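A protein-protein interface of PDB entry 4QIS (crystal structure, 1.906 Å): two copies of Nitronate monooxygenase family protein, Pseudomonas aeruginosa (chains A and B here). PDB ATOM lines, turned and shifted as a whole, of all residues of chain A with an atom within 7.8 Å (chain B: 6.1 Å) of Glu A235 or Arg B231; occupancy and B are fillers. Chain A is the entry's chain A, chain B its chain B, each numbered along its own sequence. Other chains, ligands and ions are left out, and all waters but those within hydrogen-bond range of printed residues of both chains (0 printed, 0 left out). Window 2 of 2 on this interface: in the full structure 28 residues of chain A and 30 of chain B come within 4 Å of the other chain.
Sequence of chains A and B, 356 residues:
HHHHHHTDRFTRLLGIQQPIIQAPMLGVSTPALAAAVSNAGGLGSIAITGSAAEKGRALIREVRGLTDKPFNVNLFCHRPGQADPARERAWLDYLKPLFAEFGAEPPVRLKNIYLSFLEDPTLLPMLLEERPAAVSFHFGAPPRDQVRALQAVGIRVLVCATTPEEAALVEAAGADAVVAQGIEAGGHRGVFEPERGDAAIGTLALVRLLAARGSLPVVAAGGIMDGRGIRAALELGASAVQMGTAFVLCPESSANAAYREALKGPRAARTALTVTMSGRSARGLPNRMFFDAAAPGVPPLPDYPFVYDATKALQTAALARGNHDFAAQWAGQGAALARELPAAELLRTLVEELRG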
ATOM      1  N   LEU A 204      21.355 -33.062  11.121  1.00  0.00           N
ATOM      2  CA  LEU A 204      20.742 -31.756  11.291  1.00  0.00           C
ATOM      3  C   LEU A 204      19.693 -31.438  10.224  1.00  0.00           C
ATOM      4  O   LEU A 204      18.608 -30.966  10.564  1.00  0.00           O
ATOM      5  CB  LEU A 204      21.774 -30.633  11.422  1.00  0.00           C
ATOM      6  CG  LEU A 204      21.188 -29.230  11.658  1.00  0.00           C
ATOM      7  CD1 LEU A 204      21.889 -28.468  12.770  1.00  0.00           C
ATOM      8  CD2 LEU A 204      21.220 -28.417  10.383  1.00  0.00           C
ATOM      9  N   VAL A 207      16.589 -34.538  10.356  1.00  0.00           N
ATOM     10  CA  VAL A 207      15.607 -34.420  11.432  1.00  0.00           C
ATOM     11  C   VAL A 207      14.652 -33.266  11.165  1.00  0.00           C
ATOM     12  O   VAL A 207      13.442 -33.411  11.320  1.00  0.00           O
ATOM     13  CB  VAL A 207      16.259 -34.173  12.807  1.00  0.00           C
ATOM     14  CG1 VAL A 207      15.172 -33.929  13.864  1.00  0.00           C
ATOM     15  CG2 VAL A 207      17.188 -35.341  13.200  1.00  0.00           C
ATOM     16  N   ARG A 208      15.206 -32.127  10.753  1.00  0.00           N
ATOM     17  CA  ARG A 208      14.401 -30.940  10.513  1.00  0.00           C
ATOM     18  C   ARG A 208      13.390 -31.206   9.427  1.00  0.00           C
ATOM     19  O   ARG A 208      12.222 -30.864   9.563  1.00  0.00           O
ATOM     20  CB  ARG A 208      15.260 -29.733  10.147  1.00  0.00           C
ATOM     21  CG  ARG A 208      14.474 -28.419  10.201  1.00  0.00           C
ATOM     22  CD  ARG A 208      14.136 -28.054  11.655  1.00  0.00           C
ATOM     23  NE  ARG A 208      13.036 -27.103  11.724  1.00  0.00           N
ATOM     24  CZ  ARG A 208      11.782 -27.436  12.012  1.00  0.00           C
ATOM     25  NH1 ARG A 208      10.842 -26.507  12.026  1.00  0.00           N
ATOM     26  NH2 ARG A 208      11.464 -28.692  12.291  1.00  0.00           N
ATOM     27  N   ALA A 211      10.644 -33.658  10.781  1.00  0.00           N
ATOM     28  CA  ALA A 211       9.808 -33.031  11.800  1.00  0.00           C
ATOM     29  C   ALA A 211       8.970 -31.888  11.231  1.00  0.00           C
ATOM     30  O   ALA A 211       7.866 -31.612  11.723  1.00  0.00           O
ATOM     31  CB  ALA A 211      10.641 -32.537  12.978  1.00  0.00           C
ATOM     32  N   ARG A 228      23.737 -31.934  25.255  1.00  0.00           N
ATOM     33  CA  ARG A 228      23.645 -30.812  24.332  1.00  0.00           C
ATOM     34  C   ARG A 228      23.244 -31.307  22.957  1.00  0.00           C
ATOM     35  O   ARG A 228      22.464 -30.658  22.260  1.00  0.00           O
ATOM     36  CB  ARG A 228      24.967 -30.049  24.270  1.00  0.00           C
ATOM     37  CG  ARG A 228      25.209 -29.111  25.446  1.00  0.00           C
ATOM     38  CD  ARG A 228      26.571 -28.454  25.291  1.00  0.00           C
ATOM     39  NE  ARG A 228      26.760 -27.330  26.197  1.00  0.00           N
ATOM     40  CZ  ARG A 228      26.563 -26.063  25.852  1.00  0.00           C
ATOM     41  NH1 ARG A 228      26.175 -25.769  24.620  1.00  0.00           N
ATOM     42  NH2 ARG A 228      26.759 -25.095  26.735  1.00  0.00           N
ATOM     43  N   GLY A 229      23.756 -32.472  22.579  1.00  0.00           N
ATOM     44  CA  GLY A 229      23.361 -33.096  21.327  1.00  0.00           C
ATOM     45  C   GLY A 229      21.892 -33.490  21.311  1.00  0.00           C
ATOM     46  O   GLY A 229      21.233 -33.370  20.281  1.00  0.00           O
ATOM     47  N   ILE A 230      21.378 -33.961  22.448  1.00  0.00           N
ATOM     48  CA  ILE A 230      19.961 -34.315  22.560  1.00  0.00           C
ATOM     49  C   ILE A 230      19.056 -33.075  22.479  1.00  0.00           C
ATOM     50  O   ILE A 230      18.031 -33.096  21.805  1.00  0.00           O
ATOM     51  CB  ILE A 230      19.653 -35.068  23.860  1.00  0.00           C
ATOM     52  CG1 ILE A 230      20.510 -36.343  23.978  1.00  0.00           C
ATOM     53  CG2 ILE A 230      18.169 -35.432  23.920  1.00  0.00           C
ATOM     54  CD1 ILE A 230      20.403 -37.021  25.331  1.00  0.00           C
ATOM     55  N   ARG A 231      19.457 -32.005  23.161  1.00  0.00           N
ATOM     56  CA  ARG A 231      18.720 -30.743  23.164  1.00  0.00           C
ATOM     57  C   ARG A 231      18.658 -30.173  21.765  1.00  0.00           C
ATOM     58  O   ARG A 231      17.635 -29.622  21.341  1.00  0.00           O
ATOM     59  CB  ARG A 231      19.400 -29.730  24.090  1.00  0.00           C
ATOM     60  CG  ARG A 231      19.426 -30.138  25.560  1.00  0.00           C
ATOM     61  CD  ARG A 231      20.209 -29.131  26.412  1.00  0.00           C
ATOM     62  NE  ARG A 231      19.637 -27.790  26.341  1.00  0.00           N
ATOM     63  CZ  ARG A 231      18.664 -27.336  27.130  1.00  0.00           C
ATOM     64  NH1 ARG A 231      18.135 -28.110  28.071  1.00  0.00           N
ATOM     65  NH2 ARG A 231      18.219 -26.098  26.981  1.00  0.00           N
ATOM     66  N   ALA A 232      19.765 -30.307  21.047  1.00  0.00           N
ATOM     67  CA  ALA A 232      19.842 -29.832  19.671  1.00  0.00           C
ATOM     68  C   ALA A 232      18.828 -30.554  18.789  1.00  0.00           C
ATOM     69  O   ALA A 232      18.088 -29.925  18.039  1.00  0.00           O
ATOM     70  CB  ALA A 232      21.251 -30.030  19.131  1.00  0.00           C
ATOM     71  N   ALA A 233      18.791 -31.880  18.901  1.00  0.00           N
ATOM     72  CA  ALA A 233      17.860 -32.688  18.121  1.00  0.00           C
ATOM     73  C   ALA A 233      16.425 -32.312  18.443  1.00  0.00           C
ATOM     74  O   ALA A 233      15.572 -32.316  17.556  1.00  0.00           O
ATOM     75  CB  ALA A 233      18.081 -34.156  18.390  1.00  0.00           C
ATOM     76  N   LEU A 234      16.166 -32.005  19.716  1.00  0.00           N
ATOM     77  CA  LEU A 234      14.828 -31.618  20.150  1.00  0.00           C
ATOM     78  C   LEU A 234      14.491 -30.249  19.584  1.00  0.00           C
ATOM     79  O   LEU A 234      13.367 -30.018  19.149  1.00  0.00           O
ATOM     80  CB  LEU A 234      14.701 -31.627  21.682  1.00  0.00           C
ATOM     81  CG  LEU A 234      14.900 -32.964  22.395  1.00  0.00           C
ATOM     82  CD1 LEU A 234      14.757 -32.764  23.891  1.00  0.00           C
ATOM     83  CD2 LEU A 234      13.923 -33.986  21.913  1.00  0.00           C
ATOM     84  N   GLU A 235      15.469 -29.350  19.552  1.00  0.00           N
ATOM     85  CA  GLU A 235      15.233 -28.057  18.914  1.00  0.00           C
ATOM     86  C   GLU A 235      14.862 -28.236  17.445  1.00  0.00           C
ATOM     87  O   GLU A 235      14.102 -27.443  16.897  1.00  0.00           O
ATOM     88  CB  GLU A 235      16.434 -27.116  19.071  1.00  0.00           C
ATOM     89  CG  GLU A 235      16.621 -26.559  20.497  1.00  0.00           C
ATOM     90  CD  GLU A 235      15.549 -25.533  20.893  1.00  0.00           C
ATOM     91  OE1 GLU A 235      14.722 -25.179  20.036  1.00  0.00           O
ATOM     92  OE2 GLU A 235      15.535 -25.085  22.065  1.00  0.00           O
ATOM     93  N   LEU A 236      15.377 -29.298  16.821  1.00  0.00           N
ATOM     94  CA  LEU A 236      15.115 -29.587  15.403  1.00  0.00           C
ATOM     95  C   LEU A 236      13.757 -30.229  15.166  1.00  0.00           C
ATOM     96  O   LEU A 236      13.350 -30.411  14.018  1.00  0.00           O
ATOM     97  CB  LEU A 236      16.196 -30.500  14.821  1.00  0.00           C
ATOM     98  CG  LEU A 236      17.597 -29.907  14.602  1.00  0.00           C
ATOM     99  CD1 LEU A 236      18.597 -30.976  14.115  1.00  0.00           C
ATOM    100  CD2 LEU A 236      17.549 -28.747  13.624  1.00  0.00           C
ATOM    101  N   GLY A 237      13.084 -30.611  16.250  1.00  0.00           N
ATOM    102  CA  GLY A 237      11.740 -31.148  16.165  1.00  0.00           C
ATOM    103  C   GLY A 237      11.639 -32.627  16.472  1.00  0.00           C
ATOM    104  O   GLY A 237      10.558 -33.220  16.332  1.00  0.00           O
ATOM    105  N   ALA A 238      12.755 -33.230  16.880  1.00  0.00           N
ATOM    106  CA  ALA A 238      12.754 -34.637  17.268  1.00  0.00           C
ATOM    107  C   ALA A 238      11.924 -34.803  18.531  1.00  0.00           C
ATOM    108  O   ALA A 238      11.893 -33.913  19.375  1.00  0.00           O
ATOM    109  CB  ALA A 238      14.179 -35.135  17.507  1.00  0.00           C
ATOM    110  N   ASP B 226      16.099 -22.165   9.377  1.00  0.00           N
ATOM    111  CA  ASP B 226      15.105 -21.506  10.218  1.00  0.00           C
ATOM    112  C   ASP B 226      15.630 -21.273  11.635  1.00  0.00           C
ATOM    113  O   ASP B 226      16.788 -21.583  11.940  1.00  0.00           O
ATOM    114  CB  ASP B 226      13.785 -22.300  10.241  1.00  0.00           C
ATOM    115  CG  ASP B 226      13.974 -23.762  10.618  1.00  0.00           C
ATOM    116  OD1 ASP B 226      14.878 -24.074  11.433  1.00  0.00           O
ATOM    117  OD2 ASP B 226      13.203 -24.603  10.103  1.00  0.00           O
ATOM    118  N   GLY B 227      14.774 -20.718  12.491  1.00  0.00           N
ATOM    119  CA  GLY B 227      15.130 -20.427  13.864  1.00  0.00           C
ATOM    120  C   GLY B 227      15.379 -21.681  14.676  1.00  0.00           C
ATOM    121  O   GLY B 227      16.205 -21.675  15.577  1.00  0.00           O
ATOM    122  N   ARG B 228      14.673 -22.758  14.366  1.00  0.00           N
ATOM    123  CA  ARG B 228      14.902 -24.011  15.083  1.00  0.00           C
ATOM    124  C   ARG B 228      16.309 -24.534  14.829  1.00  0.00           C
ATOM    125  O   ARG B 228      16.996 -24.982  15.761  1.00  0.00           O
ATOM    126  CB  ARG B 228      13.861 -25.059  14.700  1.00  0.00           C
ATOM    127  CG  ARG B 228      12.607 -24.994  15.549  1.00  0.00           C
ATOM    128  CD  ARG B 228      11.531 -25.923  15.028  1.00  0.00           C
ATOM    129  NE  ARG B 228      10.364 -25.923  15.902  1.00  0.00           N
ATOM    130  CZ  ARG B 228      10.176 -26.794  16.890  1.00  0.00           C
ATOM    131  NH1 ARG B 228      11.071 -27.745  17.121  1.00  0.00           N
ATOM    132  NH2 ARG B 228       9.088 -26.720  17.642  1.00  0.00           N
ATOM    133  N   GLY B 229      16.724 -24.470  13.566  1.00  0.00           N
ATOM    134  CA  GLY B 229      18.072 -24.815  13.174  1.00  0.00           C
ATOM    135  C   GLY B 229      19.099 -23.980  13.904  1.00  0.00           C
ATOM    136  O   GLY B 229      20.073 -24.519  14.417  1.00  0.00           O
ATOM    137  N   ILE B 230      18.885 -22.669  13.966  1.00  0.00           N
ATOM    138  CA  ILE B 230      19.824 -21.788  14.645  1.00  0.00           C
ATOM    139  C   ILE B 230      19.908 -22.135  16.121  1.00  0.00           C
ATOM    140  O   ILE B 230      21.003 -22.181  16.698  1.00  0.00           O
ATOM    141  CB  ILE B 230      19.430 -20.305  14.489  1.00  0.00           C
ATOM    142  CG1 ILE B 230      19.411 -19.910  13.008  1.00  0.00           C
ATOM    143  CG2 ILE B 230      20.373 -19.406  15.295  1.00  0.00           C
ATOM    144  CD1 ILE B 230      18.878 -18.507  12.750  1.00  0.00           C
ATOM    145  N   ARG B 231      18.745 -22.396  16.716  1.00  0.00           N
ATOM    146  CA  ARG B 231      18.651 -22.790  18.116  1.00  0.00           C
ATOM    147  C   ARG B 231      19.425 -24.079  18.353  1.00  0.00           C
ATOM    148  O   ARG B 231      20.170 -24.206  19.334  1.00  0.00           O
ATOM    149  CB  ARG B 231      17.186 -22.984  18.530  1.00  0.00           C
ATOM    150  CG  ARG B 231      16.387 -21.683  18.671  1.00  0.00           C
ATOM    151  CD  ARG B 231      14.998 -21.926  19.268  1.00  0.00           C
ATOM    152  NE  ARG B 231      14.692 -20.946  20.304  1.00  0.00           N
ATOM    153  CZ  ARG B 231      14.662 -21.215  21.603  1.00  0.00           C
ATOM    154  NH1 ARG B 231      14.890 -22.447  22.025  1.00  0.00           N
ATOM    155  NH2 ARG B 231      14.383 -20.259  22.479  1.00  0.00           N
ATOM    156  N   ALA B 232      19.246 -25.032  17.444  1.00  0.00           N
ATOM    157  CA  ALA B 232      19.929 -26.314  17.542  1.00  0.00           C
ATOM    158  C   ALA B 232      21.448 -26.149  17.468  1.00  0.00           C
ATOM    159  O   ALA B 232      22.177 -26.763  18.253  1.00  0.00           O
ATOM    160  CB  ALA B 232      19.428 -27.260  16.480  1.00  0.00           C
ATOM    161  N   ALA B 233      21.912 -25.321  16.531  1.00  0.00           N
ATOM    162  CA  ALA B 233      23.338 -25.014  16.382  1.00  0.00           C
ATOM    163  C   ALA B 233      23.942 -24.404  17.645  1.00  0.00           C
ATOM    164  O   ALA B 233      25.064 -24.744  18.028  1.00  0.00           O
ATOM    165  CB  ALA B 233      23.566 -24.096  15.185  1.00  0.00           C
ATOM    166  N   LEU B 234      23.202 -23.502  18.287  1.00  0.00           N
ATOM    167  CA  LEU B 234      23.658 -22.896  19.536  1.00  0.00           C
ATOM    168  C   LEU B 234      23.749 -23.932  20.662  1.00  0.00           C
ATOM    169  O   LEU B 234      24.699 -23.926  21.438  1.00  0.00           O
ATOM    170  CB  LEU B 234      22.751 -21.726  19.935  1.00  0.00           C
ATOM    171  CG  LEU B 234      23.046 -20.343  19.341  1.00  0.00           C
ATOM    172  CD1 LEU B 234      23.746 -20.412  17.975  1.00  0.00           C
ATOM    173  CD2 LEU B 234      21.769 -19.518  19.237  1.00  0.00           C
ATOM    174  N   GLU B 235      22.779 -24.832  20.739  1.00  0.00           N
ATOM    175  CA  GLU B 235      22.817 -25.907  21.742  1.00  0.00           C
ATOM    176  C   GLU B 235      24.057 -26.772  21.573  1.00  0.00           C
ATOM    177  O   GLU B 235      24.649 -27.229  22.550  1.00  0.00           O
ATOM    178  CB  GLU B 235      21.567 -26.795  21.655  1.00  0.00           C
ATOM    179  CG  GLU B 235      20.313 -26.249  22.355  1.00  0.00           C
ATOM    180  CD  GLU B 235      20.534 -25.889  23.827  1.00  0.00           C
ATOM    181  OE1 GLU B 235      21.378 -26.515  24.508  1.00  0.00           O
ATOM    182  OE2 GLU B 235      19.853 -24.962  24.310  1.00  0.00           O
ATOM    183  N   LEU B 236      24.439 -27.006  20.322  1.00  0.00           N
ATOM    184  CA  LEU B 236      25.647 -27.769  20.023  1.00  0.00           C
ATOM    185  C   LEU B 236      26.910 -27.029  20.457  1.00  0.00           C
ATOM    186  O   LEU B 236      27.978 -27.637  20.549  1.00  0.00           O
ATOM    187  CB  LEU B 236      25.725 -28.120  18.530  1.00  0.00           C
ATOM    188  CG  LEU B 236      24.613 -29.066  18.087  1.00  0.00           C
ATOM    189  CD1 LEU B 236      24.570 -29.265  16.553  1.00  0.00           C
ATOM    190  CD2 LEU B 236      24.756 -30.390  18.836  1.00  0.00           C
ATOM    191  N   GLU B 353      11.973 -16.382  15.003  1.00  0.00           N
ATOM    192  CA  GLU B 353      11.925 -17.828  15.189  1.00  0.00           C
ATOM    193  C   GLU B 353      13.002 -18.263  16.172  1.00  0.00           C
ATOM    194  O   GLU B 353      12.794 -19.173  16.974  1.00  0.00           O
ATOM    195  CB  GLU B 353      12.130 -18.540  13.854  1.00  0.00           C
ATOM    196  CG  GLU B 353      11.046 -18.285  12.819  1.00  0.00           C
ATOM    197  CD  GLU B 353      11.368 -18.929  11.480  1.00  0.00           C
ATOM    198  OE1 GLU B 353      12.568 -19.171  11.210  1.00  0.00           O
ATOM    199  OE2 GLU B 353      10.429 -19.196  10.698  1.00  0.00           O
ATOM    200  N   LEU B 354      14.158 -17.611  16.093  1.00  0.00           N
ATOM    201  CA  LEU B 354      15.234 -17.831  17.044  1.00  0.00           C
ATOM    202  C   LEU B 354      14.751 -17.525  18.466  1.00  0.00           C
ATOM    203  O   LEU B 354      15.202 -18.153  19.431  1.00  0.00           O
ATOM    204  CB  LEU B 354      16.449 -16.970  16.685  1.00  0.00           C
ATOM    205  CG  LEU B 354      17.546 -16.836  17.752  1.00  0.00           C
ATOM    206  CD1 LEU B 354      18.256 -18.176  17.987  1.00  0.00           C
ATOM    207  CD2 LEU B 354      18.534 -15.728  17.389  1.00  0.00           C
ATOM    208  N   ARG B 355      13.815 -16.580  18.570  1.00  0.00           N
ATOM    209  CA  ARG B 355      13.200 -16.163  19.836  1.00  0.00           C
ATOM    210  C   ARG B 355      14.174 -15.414  20.733  1.00  0.00           C
ATOM    211  O   ARG B 355      13.810 -14.410  21.348  1.00  0.00           O
ATOM    212  CB  ARG B 355      12.574 -17.346  20.593  1.00  0.00           C
ATOM    213  CG  ARG B 355      11.845 -18.335  19.702  1.00  0.00           C
ATOM    214  CD  ARG B 355      11.068 -19.321  20.518  1.00  0.00           C
ATOM    215  NE  ARG B 355       9.869 -18.700  21.064  1.00  0.00           N
ATOM    216  CZ  ARG B 355       9.291 -19.065  22.203  1.00  0.00           C
ATOM    217  NH1 ARG B 355       9.813 -20.050  22.927  1.00  0.00           N
ATOM    218  NH2 ARG B 355       8.195 -18.440  22.621  1.00  0.00           N
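The backbone NH (N) of Gly B229 is in hydrogen-bond range of the side-chain carboxylate (OD1) of Asp B226 (2.8 Å). The backbone carbonyl oxygen (O) of Leu A236 sits at hydrogen-bond distance from the guanidinium group (NH2) of Arg A208. OD1 of Asp B226 sits at hydrogen-bond distance from N of Arg B228, at 3.2 Å. O of Leu B354 lies within hydrogen-bond range of NE of Arg B231, at 3.0 Å.
Of the printed residues of chain B, Glu A235 touches Arg B228, Arg B231 and Ala B232. Of chain A, only Glu A235 (2.7 Å) comes within 4 Å of Arg B231. Ala B232 touches just these residues of chain A: Ala A232 (3.4 Å), Glu A235 (3.9 Å) and Leu A236 (3.7 Å). Printed residues of chain B within 4 Å of Arg A228: Leu B234 (3.96 Å) and Glu B235 (3.0 Å). Of the printed residues of chain B, Arg A231 touches Glu B235. Of the printed residues of chain A, Glu B235 touches Arg A228 (3.0 Å), Arg A231 (2.8 Å) and Ala A232 (3.99 Å). Glu B353 touches none of the printed residues of chain A. Leu A204 touches none of the printed residues of chain B.
Arg A228 touches Leu B234, and with the chains exchanged Leu A234 touches Arg B228. Arg A228 touches Glu B235, and with the chains exchanged Glu A235 touches Arg B228. Ala A232 touches its own counterpart, Ala B232. Ala A232 touches Leu B236, and with the chains exchanged Leu A236 touches Ala B232. 9 positions are printed for both chains.
Among the printed residues, merely in contact across the chains: Arg A208 with Arg B228, Ala A232 with Ala B232, Ala A232 with Leu B236, Gly A237 with Arg B228, Leu A236 with Ala B232, Leu A234 with Arg B228, Glu A235 with Ala B232, Gly A229 with Leu B236, Arg A228 with Leu B234, Leu A236 with Gly B229 and Ala A232 with Glu B235.
Of the 15 printed residues of chain A, 9 touch a printed residue of chain B. Hydrophobic or aromatic side chains of chain A within 4 Å of the printed part of chain B: Ala A232 and Leu A236. Among the printed residues, 16 pairs touch across the chains. Among the printed residues, Asp or Glu carboxylates within 4 Å of a Lys or Arg side-chain nitrogen of the other chain: Arg A208 with Asp B226 (3.0 Å), Arg A231 with Glu B235 (2.8 Å) and Glu A235 with Arg B231 (2.7 Å).
The side-chain carboxylate (OD2) of Asp B226 is in salt-bridge range of the guanidinium group (NE) of Arg A208, 3.0 Å away. The side-chain carboxylate of Glu A235 lies within salt-bridge range of the guanidinium group of Arg B231, at 2.7 Å. NH1 of Arg A228 sits at hydrogen-bond distance from O of Glu B235 (3.0 Å). The side-chain carboxylate of Glu B235 lies within salt-bridge range of the guanidinium group of Arg A231 (2.8 Å). NH1 of Arg B228 is in hydrogen-bond range of O of Glu A235, at 3.1 Å.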
